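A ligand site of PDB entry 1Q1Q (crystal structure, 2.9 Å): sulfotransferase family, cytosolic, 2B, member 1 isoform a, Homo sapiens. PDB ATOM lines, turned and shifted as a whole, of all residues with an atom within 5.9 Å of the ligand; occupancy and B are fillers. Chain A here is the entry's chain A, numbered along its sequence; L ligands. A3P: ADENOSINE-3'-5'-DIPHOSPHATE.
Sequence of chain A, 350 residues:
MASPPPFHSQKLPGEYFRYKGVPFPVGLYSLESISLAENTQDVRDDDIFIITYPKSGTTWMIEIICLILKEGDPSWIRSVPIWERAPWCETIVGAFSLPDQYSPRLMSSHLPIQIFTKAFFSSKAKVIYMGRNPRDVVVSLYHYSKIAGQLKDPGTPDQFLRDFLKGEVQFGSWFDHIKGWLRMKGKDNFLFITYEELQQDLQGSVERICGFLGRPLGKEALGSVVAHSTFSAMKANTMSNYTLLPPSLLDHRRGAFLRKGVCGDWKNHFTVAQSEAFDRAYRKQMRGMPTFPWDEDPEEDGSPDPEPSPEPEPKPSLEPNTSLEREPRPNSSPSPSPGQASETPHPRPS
O of Ser 229 is in hydrogen-bond range of NE1 of Trp 60 (3.5 Å). NE2 of Gln 199 is in hydrogen-bond range of O of Gly 261 (2.8 Å). NH1 of Arg 132 is in hydrogen-bond range of O of Lys 55 (3.0 Å). The side-chain amide nitrogen (NE2) of Gln 199 sits at hydrogen-bond distance from the side-chain hydroxyl (OH) of Tyr 195, 3.1 Å away. The side-chain hydroxyl of Ser 56 lies within hydrogen-bond range of the backbone carbonyl oxygen of Tyr 53, 2.9 Å away. OG1 of Thr 58 is in hydrogen-bond range of OG1 of Thr 52, at 2.6 Å. The guanidinium group (NH2) of Arg 132 lies within hydrogen-bond range of the backbone carbonyl oxygen (O) of Val 262 (3.3 Å). NZ of Lys 260 lies within salt-bridge range of OD2 of Asp 265 (3.6 Å).
An oxygen (O3P) of the ligand is in salt-bridge range of the guanidinium group (NH2) of Arg 132 (3.3 Å). The guanidinium group (NE) of Arg 259 lies within salt-bridge range of an oxygen (O1P) of the ligand, at 3.0 Å. O5P of the ligand is in hydrogen-bond range of N of Thr 59, 3.0 Å away. The backbone carbonyl oxygen of Ser 229 lies within hydrogen-bond range of a nitrogen (N6) of the ligand. N of Ser 56 sits at hydrogen-bond distance from O6P of the ligand (3.3 Å). The side-chain sulfur (SD) of Met 234 lies within hydrogen-bond range of a nitrogen (N6) of the ligand, at 3.4 Å. N of Lys 260 sits at hydrogen-bond distance from O2P of the ligand (2.9 Å). O6P of the ligand is in hydrogen-bond range of N of Gly 57 (3.1 Å). O6P of the ligand lies within hydrogen-bond range of N of Thr 58, at 2.8 Å. OG of Ser 140 lies within hydrogen-bond range of O1P of the ligand (2.7 Å). O4P of the ligand is in salt-bridge range of NZ of Lys 55, at 3.0 Å. The side-chain hydroxyl (OG1) of Thr 59 is in hydrogen-bond range of an oxygen (O5P) of the ligand (2.5 Å). The backbone NH (N) of Arg 259 lies close to an oxygen (O2P) of the ligand (3.3 Å). O6P of the ligand is in hydrogen-bond range of N of Lys 55. O2P of the ligand sits at hydrogen-bond distance from N of Gly 261 (3.1 Å). A nitrogen (N3) of the ligand lies within hydrogen-bond range of the side-chain hydroxyl (OH) of Tyr 195. An oxygen (O6P) of the ligand lies within hydrogen-bond range of the side-chain hydroxyl of Thr 58, 2.8 Å away.
CD1 of Trp 60 touches N6 of the ligand, 3.4 Å away. Gln 199 touches the ligand (NE2 to C2, 3.7 Å). C of Thr 230 touches N6 of the ligand (3.8 Å). Phe 231 touches the ligand (N to N6, 3.6 Å). Phe 257 touches the ligand. Leu 258 touches the ligand (CA to O2', 3.4 Å). Of the 31 residues printed, 19 come within 4 Å of the ligand.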
ATOM      1  N   THR A  52     -25.089  21.318   8.035  1.00  0.00           N
ATOM      2  CA  THR A  52     -25.058  19.974   7.523  1.00  0.00           C
ATOM      3  C   THR A  52     -25.943  19.058   8.346  1.00  0.00           C
ATOM      4  O   THR A  52     -26.382  19.424   9.437  1.00  0.00           O
ATOM      5  CB  THR A  52     -23.651  19.379   7.624  1.00  0.00           C
ATOM      6  OG1 THR A  52     -23.270  19.326   9.013  1.00  0.00           O
ATOM      7  CG2 THR A  52     -22.648  20.221   6.852  1.00  0.00           C
ATOM      8  N   TYR A  53     -26.193  17.874   7.804  1.00  0.00           N
ATOM      9  CA  TYR A  53     -26.948  16.825   8.485  1.00  0.00           C
ATOM     10  C   TYR A  53     -25.815  15.977   9.116  1.00  0.00           C
ATOM     11  O   TYR A  53     -24.827  15.642   8.449  1.00  0.00           O
ATOM     12  CB  TYR A  53     -27.733  15.974   7.485  1.00  0.00           C
ATOM     13  CG  TYR A  53     -28.553  14.876   8.134  1.00  0.00           C
ATOM     14  CD1 TYR A  53     -29.794  15.142   8.697  1.00  0.00           C
ATOM     15  CD2 TYR A  53     -28.088  13.559   8.188  1.00  0.00           C
ATOM     16  CE1 TYR A  53     -30.559  14.138   9.295  1.00  0.00           C
ATOM     17  CE2 TYR A  53     -28.840  12.545   8.780  1.00  0.00           C
ATOM     18  CZ  TYR A  53     -30.073  12.842   9.344  1.00  0.00           C
ATOM     19  OH  TYR A  53     -30.840  11.871   9.938  1.00  0.00           O
ATOM     20  N   PRO A  54     -25.933  15.632  10.399  1.00  0.00           N
ATOM     21  CA  PRO A  54     -24.907  14.832  11.067  1.00  0.00           C
ATOM     22  C   PRO A  54     -24.207  13.781  10.196  1.00  0.00           C
ATOM     23  O   PRO A  54     -24.806  13.204   9.293  1.00  0.00           O
ATOM     24  CB  PRO A  54     -25.666  14.198  12.221  1.00  0.00           C
ATOM     25  CG  PRO A  54     -26.569  15.312  12.633  1.00  0.00           C
ATOM     26  CD  PRO A  54     -27.089  15.835  11.302  1.00  0.00           C
ATOM     27  N   LYS A  55     -22.929  13.568  10.478  1.00  0.00           N
ATOM     28  CA  LYS A  55     -22.112  12.572   9.788  1.00  0.00           C
ATOM     29  C   LYS A  55     -21.866  12.860   8.318  1.00  0.00           C
ATOM     30  O   LYS A  55     -21.424  11.989   7.563  1.00  0.00           O
ATOM     31  CB  LYS A  55     -22.754  11.192   9.968  1.00  0.00           C
ATOM     32  CG  LYS A  55     -23.484  11.008  11.291  1.00  0.00           C
ATOM     33  CD  LYS A  55     -22.733  11.607  12.478  1.00  0.00           C
ATOM     34  CE  LYS A  55     -21.313  11.044  12.646  1.00  0.00           C
ATOM     35  NZ  LYS A  55     -20.602  11.601  13.844  1.00  0.00           N
ATOM     36  N   SER A  56     -22.147  14.094   7.900  1.00  0.00           N
ATOM     37  CA  SER A  56     -21.921  14.455   6.509  1.00  0.00           C
ATOM     38  C   SER A  56     -20.497  14.980   6.306  1.00  0.00           C
ATOM     39  O   SER A  56     -20.060  15.189   5.173  1.00  0.00           O
ATOM     40  CB  SER A  56     -22.947  15.496   6.050  1.00  0.00           C
ATOM     41  OG  SER A  56     -24.187  14.877   5.749  1.00  0.00           O
ATOM     42  N   GLY A  57     -19.776  15.165   7.419  1.00  0.00           N
ATOM     43  CA  GLY A  57     -18.418  15.665   7.351  1.00  0.00           C
ATOM     44  C   GLY A  57     -18.376  17.130   7.758  1.00  0.00           C
ATOM     45  O   GLY A  57     -17.680  17.946   7.139  1.00  0.00           O
ATOM     46  N   THR A  58     -19.128  17.467   8.799  1.00  0.00           N
ATOM     47  CA  THR A  58     -19.157  18.841   9.282  1.00  0.00           C
ATOM     48  C   THR A  58     -17.755  19.206   9.706  1.00  0.00           C
ATOM     49  O   THR A  58     -17.173  20.194   9.238  1.00  0.00           O
ATOM     50  CB  THR A  58     -20.034  18.982  10.523  1.00  0.00           C
ATOM     51  OG1 THR A  58     -21.283  18.325  10.318  1.00  0.00           O
ATOM     52  CG2 THR A  58     -20.269  20.455  10.816  1.00  0.00           C
ATOM     53  N   THR A  59     -17.245  18.371  10.605  1.00  0.00           N
ATOM     54  CA  THR A  59     -15.908  18.480  11.169  1.00  0.00           C
ATOM     55  C   THR A  59     -14.914  18.853  10.075  1.00  0.00           C
ATOM     56  O   THR A  59     -14.244  19.869  10.170  1.00  0.00           O
ATOM     57  CB  THR A  59     -15.502  17.151  11.849  1.00  0.00           C
ATOM     58  OG1 THR A  59     -16.471  16.802  12.854  1.00  0.00           O
ATOM     59  CG2 THR A  59     -14.151  17.282  12.513  1.00  0.00           C
ATOM     60  N   TRP A  60     -14.835  18.058   9.026  1.00  0.00           N
ATOM     61  CA  TRP A  60     -13.915  18.344   7.921  1.00  0.00           C
ATOM     62  C   TRP A  60     -13.981  19.830   7.527  1.00  0.00           C
ATOM     63  O   TRP A  60     -12.959  20.514   7.509  1.00  0.00           O
ATOM     64  CB  TRP A  60     -14.267  17.488   6.709  1.00  0.00           C
ATOM     65  CG  TRP A  60     -13.236  17.481   5.620  1.00  0.00           C
ATOM     66  CD1 TRP A  60     -12.134  18.264   5.533  1.00  0.00           C
ATOM     67  CD2 TRP A  60     -13.229  16.627   4.470  1.00  0.00           C
ATOM     68  NE1 TRP A  60     -11.432  17.959   4.391  1.00  0.00           N
ATOM     69  CE2 TRP A  60     -12.077  16.952   3.721  1.00  0.00           C
ATOM     70  CE3 TRP A  60     -14.079  15.618   3.993  1.00  0.00           C
ATOM     71  CZ2 TRP A  60     -11.756  16.303   2.516  1.00  0.00           C
ATOM     72  CZ3 TRP A  60     -13.755  14.974   2.804  1.00  0.00           C
ATOM     73  CH2 TRP A  60     -12.599  15.314   2.073  1.00  0.00           C
ATOM     74  N   TRP A  88     -21.875  24.911  17.737  1.00  0.00           N
ATOM     75  CA  TRP A  88     -23.238  24.665  17.258  1.00  0.00           C
ATOM     76  C   TRP A  88     -24.281  25.543  17.936  1.00  0.00           C
ATOM     77  O   TRP A  88     -24.331  25.636  19.165  1.00  0.00           O
ATOM     78  CB  TRP A  88     -23.617  23.189  17.423  1.00  0.00           C
ATOM     79  CG  TRP A  88     -22.994  22.327  16.384  1.00  0.00           C
ATOM     80  CD1 TRP A  88     -23.451  22.087  15.118  1.00  0.00           C
ATOM     81  CD2 TRP A  88     -21.764  21.601  16.505  1.00  0.00           C
ATOM     82  NE1 TRP A  88     -22.580  21.260  14.445  1.00  0.00           N
ATOM     83  CE2 TRP A  88     -21.541  20.943  15.280  1.00  0.00           C
ATOM     84  CE3 TRP A  88     -20.836  21.442  17.538  1.00  0.00           C
ATOM     85  CZ2 TRP A  88     -20.412  20.147  15.053  1.00  0.00           C
ATOM     86  CZ3 TRP A  88     -19.719  20.656  17.317  1.00  0.00           C
ATOM     87  CH2 TRP A  88     -19.518  20.009  16.092  1.00  0.00           C
ATOM     88  N   HIS A 110     -26.920  21.805  12.622  1.00  0.00           N
ATOM     89  CA  HIS A 110     -27.494  20.608  12.015  1.00  0.00           C
ATOM     90  C   HIS A 110     -28.993  20.757  11.888  1.00  0.00           C
ATOM     91  O   HIS A 110     -29.683  19.820  11.489  1.00  0.00           O
ATOM     92  CB  HIS A 110     -27.211  19.353  12.863  1.00  0.00           C
ATOM     93  CG  HIS A 110     -25.781  18.909  12.833  1.00  0.00           C
ATOM     94  ND1 HIS A 110     -25.022  18.916  11.684  1.00  0.00           N
ATOM     95  CD2 HIS A 110     -24.970  18.457  13.823  1.00  0.00           C
ATOM     96  CE1 HIS A 110     -23.804  18.481  11.955  1.00  0.00           C
ATOM     97  NE2 HIS A 110     -23.746  18.194  13.250  1.00  0.00           N
ATOM     98  N   ARG A 132     -23.598  14.913   2.135  1.00  0.00           N
ATOM     99  CA  ARG A 132     -22.877  13.648   1.956  1.00  0.00           C
ATOM    100  C   ARG A 132     -23.803  12.553   1.430  1.00  0.00           C
ATOM    101  O   ARG A 132     -25.020  12.646   1.582  1.00  0.00           O
ATOM    102  CB  ARG A 132     -22.262  13.189   3.294  1.00  0.00           C
ATOM    103  CG  ARG A 132     -21.167  12.144   3.143  1.00  0.00           C
ATOM    104  CD  ARG A 132     -20.460  11.830   4.468  1.00  0.00           C
ATOM    105  NE  ARG A 132     -19.397  10.842   4.272  1.00  0.00           N
ATOM    106  CZ  ARG A 132     -18.747  10.203   5.254  1.00  0.00           C
ATOM    107  NH1 ARG A 132     -19.062  10.447   6.524  1.00  0.00           N
ATOM    108  NH2 ARG A 132     -17.803   9.322   4.965  1.00  0.00           N
ATOM    109  N   ASP A 136     -23.514   6.575   3.125  1.00  0.00           N
ATOM    110  CA  ASP A 136     -22.347   6.660   3.987  1.00  0.00           C
ATOM    111  C   ASP A 136     -22.738   7.312   5.305  1.00  0.00           C
ATOM    112  O   ASP A 136     -22.308   6.890   6.377  1.00  0.00           O
ATOM    113  CB  ASP A 136     -21.236   7.456   3.314  1.00  0.00           C
ATOM    114  CG  ASP A 136     -20.669   6.748   2.078  1.00  0.00           C
ATOM    115  OD1 ASP A 136     -20.384   5.526   2.168  1.00  0.00           O
ATOM    116  OD2 ASP A 136     -20.494   7.406   1.037  1.00  0.00           O
ATOM    117  N   VAL A 139     -24.013   4.633   7.602  1.00  0.00           N
ATOM    118  CA  VAL A 139     -22.956   3.786   8.106  1.00  0.00           C
ATOM    119  C   VAL A 139     -22.202   4.578   9.170  1.00  0.00           C
ATOM    120  O   VAL A 139     -21.988   4.097  10.275  1.00  0.00           O
ATOM    121  CB  VAL A 139     -21.986   3.391   7.002  1.00  0.00           C
ATOM    122  CG1 VAL A 139     -20.797   2.648   7.586  1.00  0.00           C
ATOM    123  CG2 VAL A 139     -22.695   2.520   5.987  1.00  0.00           C
ATOM    124  N   SER A 140     -21.842   5.809   8.807  1.00  0.00           N
ATOM    125  CA  SER A 140     -21.102   6.684   9.696  1.00  0.00           C
ATOM    126  C   SER A 140     -21.796   6.946  11.019  1.00  0.00           C
ATOM    127  O   SER A 140     -21.166   6.965  12.077  1.00  0.00           O
ATOM    128  CB  SER A 140     -20.814   8.010   9.023  1.00  0.00           C
ATOM    129  OG  SER A 140     -19.937   8.772   9.841  1.00  0.00           O
ATOM    130  N   LEU A 141     -23.108   7.148  10.959  1.00  0.00           N
ATOM    131  CA  LEU A 141     -23.892   7.420  12.160  1.00  0.00           C
ATOM    132  C   LEU A 141     -24.008   6.139  13.000  1.00  0.00           C
ATOM    133  O   LEU A 141     -23.993   6.188  14.225  1.00  0.00           O
ATOM    134  CB  LEU A 141     -25.285   7.939  11.777  1.00  0.00           C
ATOM    135  CG  LEU A 141     -26.293   8.203  12.909  1.00  0.00           C
ATOM    136  CD1 LEU A 141     -25.690   9.172  13.900  1.00  0.00           C
ATOM    137  CD2 LEU A 141     -27.589   8.773  12.333  1.00  0.00           C
ATOM    138  N   HIS A 143     -21.891   3.483  13.436  1.00  0.00           N
ATOM    139  CA  HIS A 143     -20.732   3.329  14.295  1.00  0.00           C
ATOM    140  C   HIS A 143     -20.699   4.406  15.392  1.00  0.00           C
ATOM    141  O   HIS A 143     -20.664   4.090  16.576  1.00  0.00           O
ATOM    142  CB  HIS A 143     -19.460   3.380  13.461  1.00  0.00           C
ATOM    143  CG  HIS A 143     -19.323   2.216  12.521  1.00  0.00           C
ATOM    144  ND1 HIS A 143     -19.477   0.906  12.931  1.00  0.00           N
ATOM    145  CD2 HIS A 143     -19.025   2.165  11.201  1.00  0.00           C
ATOM    146  CE1 HIS A 143     -19.294   0.099  11.902  1.00  0.00           C
ATOM    147  NE2 HIS A 143     -19.014   0.840  10.841  1.00  0.00           N
ATOM    148  N   TYR A 195     -19.342  16.276   0.398  1.00  0.00           N
ATOM    149  CA  TYR A 195     -18.220  15.572   0.969  1.00  0.00           C
ATOM    150  C   TYR A 195     -17.385  15.014  -0.194  1.00  0.00           C
ATOM    151  O   TYR A 195     -16.189  15.277  -0.308  1.00  0.00           O
ATOM    152  CB  TYR A 195     -18.755  14.451   1.846  1.00  0.00           C
ATOM    153  CG  TYR A 195     -17.701  13.609   2.511  1.00  0.00           C
ATOM    154  CD1 TYR A 195     -17.261  13.885   3.799  1.00  0.00           C
ATOM    155  CD2 TYR A 195     -17.135  12.552   1.831  1.00  0.00           C
ATOM    156  CE1 TYR A 195     -16.277  13.106   4.406  1.00  0.00           C
ATOM    157  CE2 TYR A 195     -16.148  11.769   2.414  1.00  0.00           C
ATOM    158  CZ  TYR A 195     -15.725  12.049   3.693  1.00  0.00           C
ATOM    159  OH  TYR A 195     -14.750  11.263   4.254  1.00  0.00           O
ATOM    160  N   GLN A 199     -13.419  15.232  -1.127  1.00  0.00           N
ATOM    161  CA  GLN A 199     -12.750  13.941  -1.273  1.00  0.00           C
ATOM    162  C   GLN A 199     -12.063  13.814  -2.629  1.00  0.00           C
ATOM    163  O   GLN A 199     -10.949  13.293  -2.723  1.00  0.00           O
ATOM    164  CB  GLN A 199     -13.744  12.778  -1.120  1.00  0.00           C
ATOM    165  CG  GLN A 199     -13.859  12.219   0.285  1.00  0.00           C
ATOM    166  CD  GLN A 199     -12.527  11.708   0.827  1.00  0.00           C
ATOM    167  OE1 GLN A 199     -11.530  11.632   0.093  1.00  0.00           O
ATOM    168  NE2 GLN A 199     -12.507  11.343   2.113  1.00  0.00           N
ATOM    169  N   SER A 229      -5.952  19.939   6.513  1.00  0.00           N
ATOM    170  CA  SER A 229      -7.348  19.484   6.505  1.00  0.00           C
ATOM    171  C   SER A 229      -7.547  18.016   6.175  1.00  0.00           C
ATOM    172  O   SER A 229      -8.631  17.469   6.383  1.00  0.00           O
ATOM    173  CB  SER A 229      -8.173  20.324   5.514  1.00  0.00           C
ATOM    174  OG  SER A 229      -8.341  21.646   5.988  1.00  0.00           O
ATOM    175  N   THR A 230      -6.489  17.390   5.669  1.00  0.00           N
ATOM    176  CA  THR A 230      -6.508  15.984   5.306  1.00  0.00           C
ATOM    177  C   THR A 230      -6.921  15.070   6.454  1.00  0.00           C
ATOM    178  O   THR A 230      -6.643  15.369   7.625  1.00  0.00           O
ATOM    179  CB  THR A 230      -5.144  15.565   4.814  1.00  0.00           C
ATOM    180  OG1 THR A 230      -4.787  16.407   3.708  1.00  0.00           O
ATOM    181  CG2 THR A 230      -5.147  14.094   4.383  1.00  0.00           C
ATOM    182  N   PHE A 231      -7.575  13.954   6.122  1.00  0.00           N
ATOM    183  CA  PHE A 231      -8.026  13.034   7.156  1.00  0.00           C
ATOM    184  C   PHE A 231      -6.950  12.755   8.175  1.00  0.00           C
ATOM    185  O   PHE A 231      -7.075  13.131   9.347  1.00  0.00           O
ATOM    186  CB  PHE A 231      -8.491  11.704   6.554  1.00  0.00           C
ATOM    187  CG  PHE A 231      -9.066  10.761   7.584  1.00  0.00           C
ATOM    188  CD1 PHE A 231     -10.084  11.173   8.424  1.00  0.00           C
ATOM    189  CD2 PHE A 231      -8.558   9.494   7.742  1.00  0.00           C
ATOM    190  CE1 PHE A 231     -10.586  10.339   9.419  1.00  0.00           C
ATOM    191  CE2 PHE A 231      -9.061   8.651   8.735  1.00  0.00           C
ATOM    192  CZ  PHE A 231     -10.072   9.085   9.572  1.00  0.00           C
ATOM    193  N   MET A 234      -5.866  15.640  10.508  1.00  0.00           N
ATOM    194  CA  MET A 234      -6.853  15.913  11.532  1.00  0.00           C
ATOM    195  C   MET A 234      -6.952  14.827  12.594  1.00  0.00           C
ATOM    196  O   MET A 234      -7.087  15.124  13.789  1.00  0.00           O
ATOM    197  CB  MET A 234      -8.216  16.146  10.875  1.00  0.00           C
ATOM    198  CG  MET A 234      -8.214  17.348   9.937  1.00  0.00           C
ATOM    199  SD  MET A 234      -9.838  17.869   9.346  1.00  0.00           S
ATOM    200  CE  MET A 234     -10.802  17.946  10.932  1.00  0.00           C
ATOM    201  N   TYR A 242     -11.689  15.141  18.669  1.00  0.00           N
ATOM    202  CA  TYR A 242     -12.650  14.916  19.749  1.00  0.00           C
ATOM    203  C   TYR A 242     -12.191  14.054  20.928  1.00  0.00           C
ATOM    204  O   TYR A 242     -12.999  13.733  21.804  1.00  0.00           O
ATOM    205  CB  TYR A 242     -13.940  14.318  19.170  1.00  0.00           C
ATOM    206  CG  TYR A 242     -14.617  15.185  18.127  1.00  0.00           C
ATOM    207  CD1 TYR A 242     -15.760  15.918  18.428  1.00  0.00           C
ATOM    208  CD2 TYR A 242     -14.064  15.313  16.854  1.00  0.00           C
ATOM    209  CE1 TYR A 242     -16.360  16.753  17.479  1.00  0.00           C
ATOM    210  CE2 TYR A 242     -14.645  16.150  15.895  1.00  0.00           C
ATOM    211  CZ  TYR A 242     -15.783  16.865  16.219  1.00  0.00           C
ATOM    212  OH  TYR A 242     -16.357  17.671  15.257  1.00  0.00           O
ATOM    213  N   PHE A 257     -14.047   9.135  16.713  1.00  0.00           N
ATOM    214  CA  PHE A 257     -14.919  10.058  15.984  1.00  0.00           C
ATOM    215  C   PHE A 257     -14.522  10.180  14.515  1.00  0.00           C
ATOM    216  O   PHE A 257     -15.365  10.440  13.653  1.00  0.00           O
ATOM    217  CB  PHE A 257     -14.878  11.452  16.632  1.00  0.00           C
ATOM    218  CG  PHE A 257     -16.034  12.335  16.243  1.00  0.00           C
ATOM    219  CD1 PHE A 257     -17.149  12.446  17.064  1.00  0.00           C
ATOM    220  CD2 PHE A 257     -16.042  12.996  15.014  1.00  0.00           C
ATOM    221  CE1 PHE A 257     -18.264  13.182  16.667  1.00  0.00           C
ATOM    222  CE2 PHE A 257     -17.145  13.737  14.600  1.00  0.00           C
ATOM    223  CZ  PHE A 257     -18.259  13.824  15.429  1.00  0.00           C
ATOM    224  N   LEU A 258     -13.242  10.012  14.215  1.00  0.00           N
ATOM    225  CA  LEU A 258     -12.769  10.073  12.832  1.00  0.00           C
ATOM    226  C   LEU A 258     -12.463   8.659  12.430  1.00  0.00           C
ATOM    227  O   LEU A 258     -11.300   8.262  12.401  1.00  0.00           O
ATOM    228  CB  LEU A 258     -11.514  10.917  12.717  1.00  0.00           C
ATOM    229  CG  LEU A 258     -11.712  12.377  13.081  1.00  0.00           C
ATOM    230  CD1 LEU A 258     -10.493  13.168  12.618  1.00  0.00           C
ATOM    231  CD2 LEU A 258     -12.967  12.906  12.423  1.00  0.00           C
ATOM    232  N   ARG A 259     -13.521   7.922  12.100  1.00  0.00           N
ATOM    233  CA  ARG A 259     -13.465   6.508  11.712  1.00  0.00           C
ATOM    234  C   ARG A 259     -12.543   6.112  10.550  1.00  0.00           C
ATOM    235  O   ARG A 259     -11.413   5.695  10.778  1.00  0.00           O
ATOM    236  CB  ARG A 259     -14.893   6.047  11.445  1.00  0.00           C
ATOM    237  CG  ARG A 259     -15.115   4.555  11.527  1.00  0.00           C
ATOM    238  CD  ARG A 259     -16.621   4.256  11.544  1.00  0.00           C
ATOM    239  NE  ARG A 259     -17.289   4.648  10.301  1.00  0.00           N
ATOM    240  CZ  ARG A 259     -17.082   4.035   9.138  1.00  0.00           C
ATOM    241  NH1 ARG A 259     -16.237   3.023   9.071  1.00  0.00           N
ATOM    242  NH2 ARG A 259     -17.705   4.444   8.043  1.00  0.00           N
ATOM    243  N   LYS A 260     -13.035   6.219   9.321  1.00  0.00           N
ATOM    244  CA  LYS A 260     -12.215   5.850   8.158  1.00  0.00           C
ATOM    245  C   LYS A 260     -11.891   7.059   7.306  1.00  0.00           C
ATOM    246  O   LYS A 260     -10.772   7.195   6.785  1.00  0.00           O
ATOM    247  CB  LYS A 260     -12.928   4.819   7.261  1.00  0.00           C
ATOM    248  CG  LYS A 260     -13.105   3.451   7.876  1.00  0.00           C
ATOM    249  CD  LYS A 260     -13.481   2.423   6.828  1.00  0.00           C
ATOM    250  CE  LYS A 260     -12.374   2.262   5.790  1.00  0.00           C
ATOM    251  NZ  LYS A 260     -12.653   1.118   4.867  1.00  0.00           N
ATOM    252  N   GLY A 261     -12.906   7.919   7.144  1.00  0.00           N
ATOM    253  CA  GLY A 261     -12.757   9.130   6.359  1.00  0.00           C
ATOM    254  C   GLY A 261     -12.698   8.884   4.863  1.00  0.00           C
ATOM    255  O   GLY A 261     -11.942   9.557   4.151  1.00  0.00           O
ATOM    256  N   VAL A 262     -13.471   7.916   4.374  1.00  0.00           N
ATOM    257  CA  VAL A 262     -13.449   7.642   2.946  1.00  0.00           C
ATOM    258  C   VAL A 262     -14.810   7.682   2.267  1.00  0.00           C
ATOM    259  O   VAL A 262     -15.878   7.699   2.899  1.00  0.00           O
ATOM    260  CB  VAL A 262     -12.794   6.296   2.628  1.00  0.00           C
ATOM    261  CG1 VAL A 262     -11.380   6.257   3.183  1.00  0.00           C
ATOM    262  CG2 VAL A 262     -13.620   5.164   3.177  1.00  0.00           C
ATOM    263  N   ASP A 265     -17.947   3.824   1.984  1.00  0.00           N
ATOM    264  CA  ASP A 265     -17.744   2.711   2.899  1.00  0.00           C
ATOM    265  C   ASP A 265     -19.085   2.007   3.052  1.00  0.00           C
ATOM    266  O   ASP A 265     -19.194   0.954   3.681  1.00  0.00           O
ATOM    267  CB  ASP A 265     -17.274   3.203   4.262  1.00  0.00           C
ATOM    268  CG  ASP A 265     -16.880   2.073   5.194  1.00  0.00           C
ATOM    269  OD1 ASP A 265     -17.202   2.170   6.397  1.00  0.00           O
ATOM    270  OD2 ASP A 265     -16.248   1.096   4.728  1.00  0.00           O
HETATM  271  P1  A3P L   1     -16.620   8.225   8.877  1.00  0.00           P
HETATM  272  O1P A3P L   1     -17.478   7.667   9.970  1.00  0.00           O
HETATM  273  O2P A3P L   1     -15.204   8.119   9.231  1.00  0.00           O
HETATM  274  O3P A3P L   1     -16.863   7.568   7.568  1.00  0.00           O
HETATM  275  P2  A3P L   1     -19.521  14.975  11.204  1.00  0.00           P
HETATM  276  O4P A3P L   1     -20.130  14.114  12.280  1.00  0.00           O
HETATM  277  O5P A3P L   1     -18.616  15.986  11.806  1.00  0.00           O
HETATM  278  O6P A3P L   1     -20.581  15.638  10.404  1.00  0.00           O
HETATM  279  O5' A3P L   1     -18.651  14.064  10.212  1.00  0.00           O
HETATM  280  C5' A3P L   1     -18.131  12.792  10.600  1.00  0.00           C
HETATM  281  C4' A3P L   1     -17.620  12.023   9.372  1.00  0.00           C
HETATM  282  O4' A3P L   1     -16.715  12.889   8.612  1.00  0.00           O
HETATM  283  C3' A3P L   1     -16.790  10.795   9.724  1.00  0.00           C
HETATM  284  O3' A3P L   1     -17.001   9.789   8.708  1.00  0.00           O
HETATM  285  C2' A3P L   1     -15.401  11.418   9.769  1.00  0.00           C
HETATM  286  O2' A3P L   1     -14.300  10.551   9.791  1.00  0.00           O
HETATM  287  C1' A3P L   1     -15.452  12.258   8.506  1.00  0.00           C
HETATM  288  N9  A3P L   1     -14.352  13.220   8.413  1.00  0.00           N
HETATM  289  C8  A3P L   1     -13.983  14.216   9.287  1.00  0.00           C
HETATM  290  N7  A3P L   1     -12.948  14.910   8.908  1.00  0.00           N
HETATM  291  C5  A3P L   1     -12.598  14.341   7.706  1.00  0.00           C
HETATM  292  C6  A3P L   1     -11.562  14.621   6.779  1.00  0.00           C
HETATM  293  N6  A3P L   1     -10.665  15.590   6.956  1.00  0.00           N
HETATM  294  N1  A3P L   1     -11.480  13.853   5.639  1.00  0.00           N
HETATM  295  C2  A3P L   1     -12.378  12.856   5.454  1.00  0.00           C
HETATM  296  N3  A3P L   1     -13.409  12.504   6.268  1.00  0.00           N
HETATM  297  C4  A3P L   1     -13.460  13.288   7.383  1.00  0.00           C
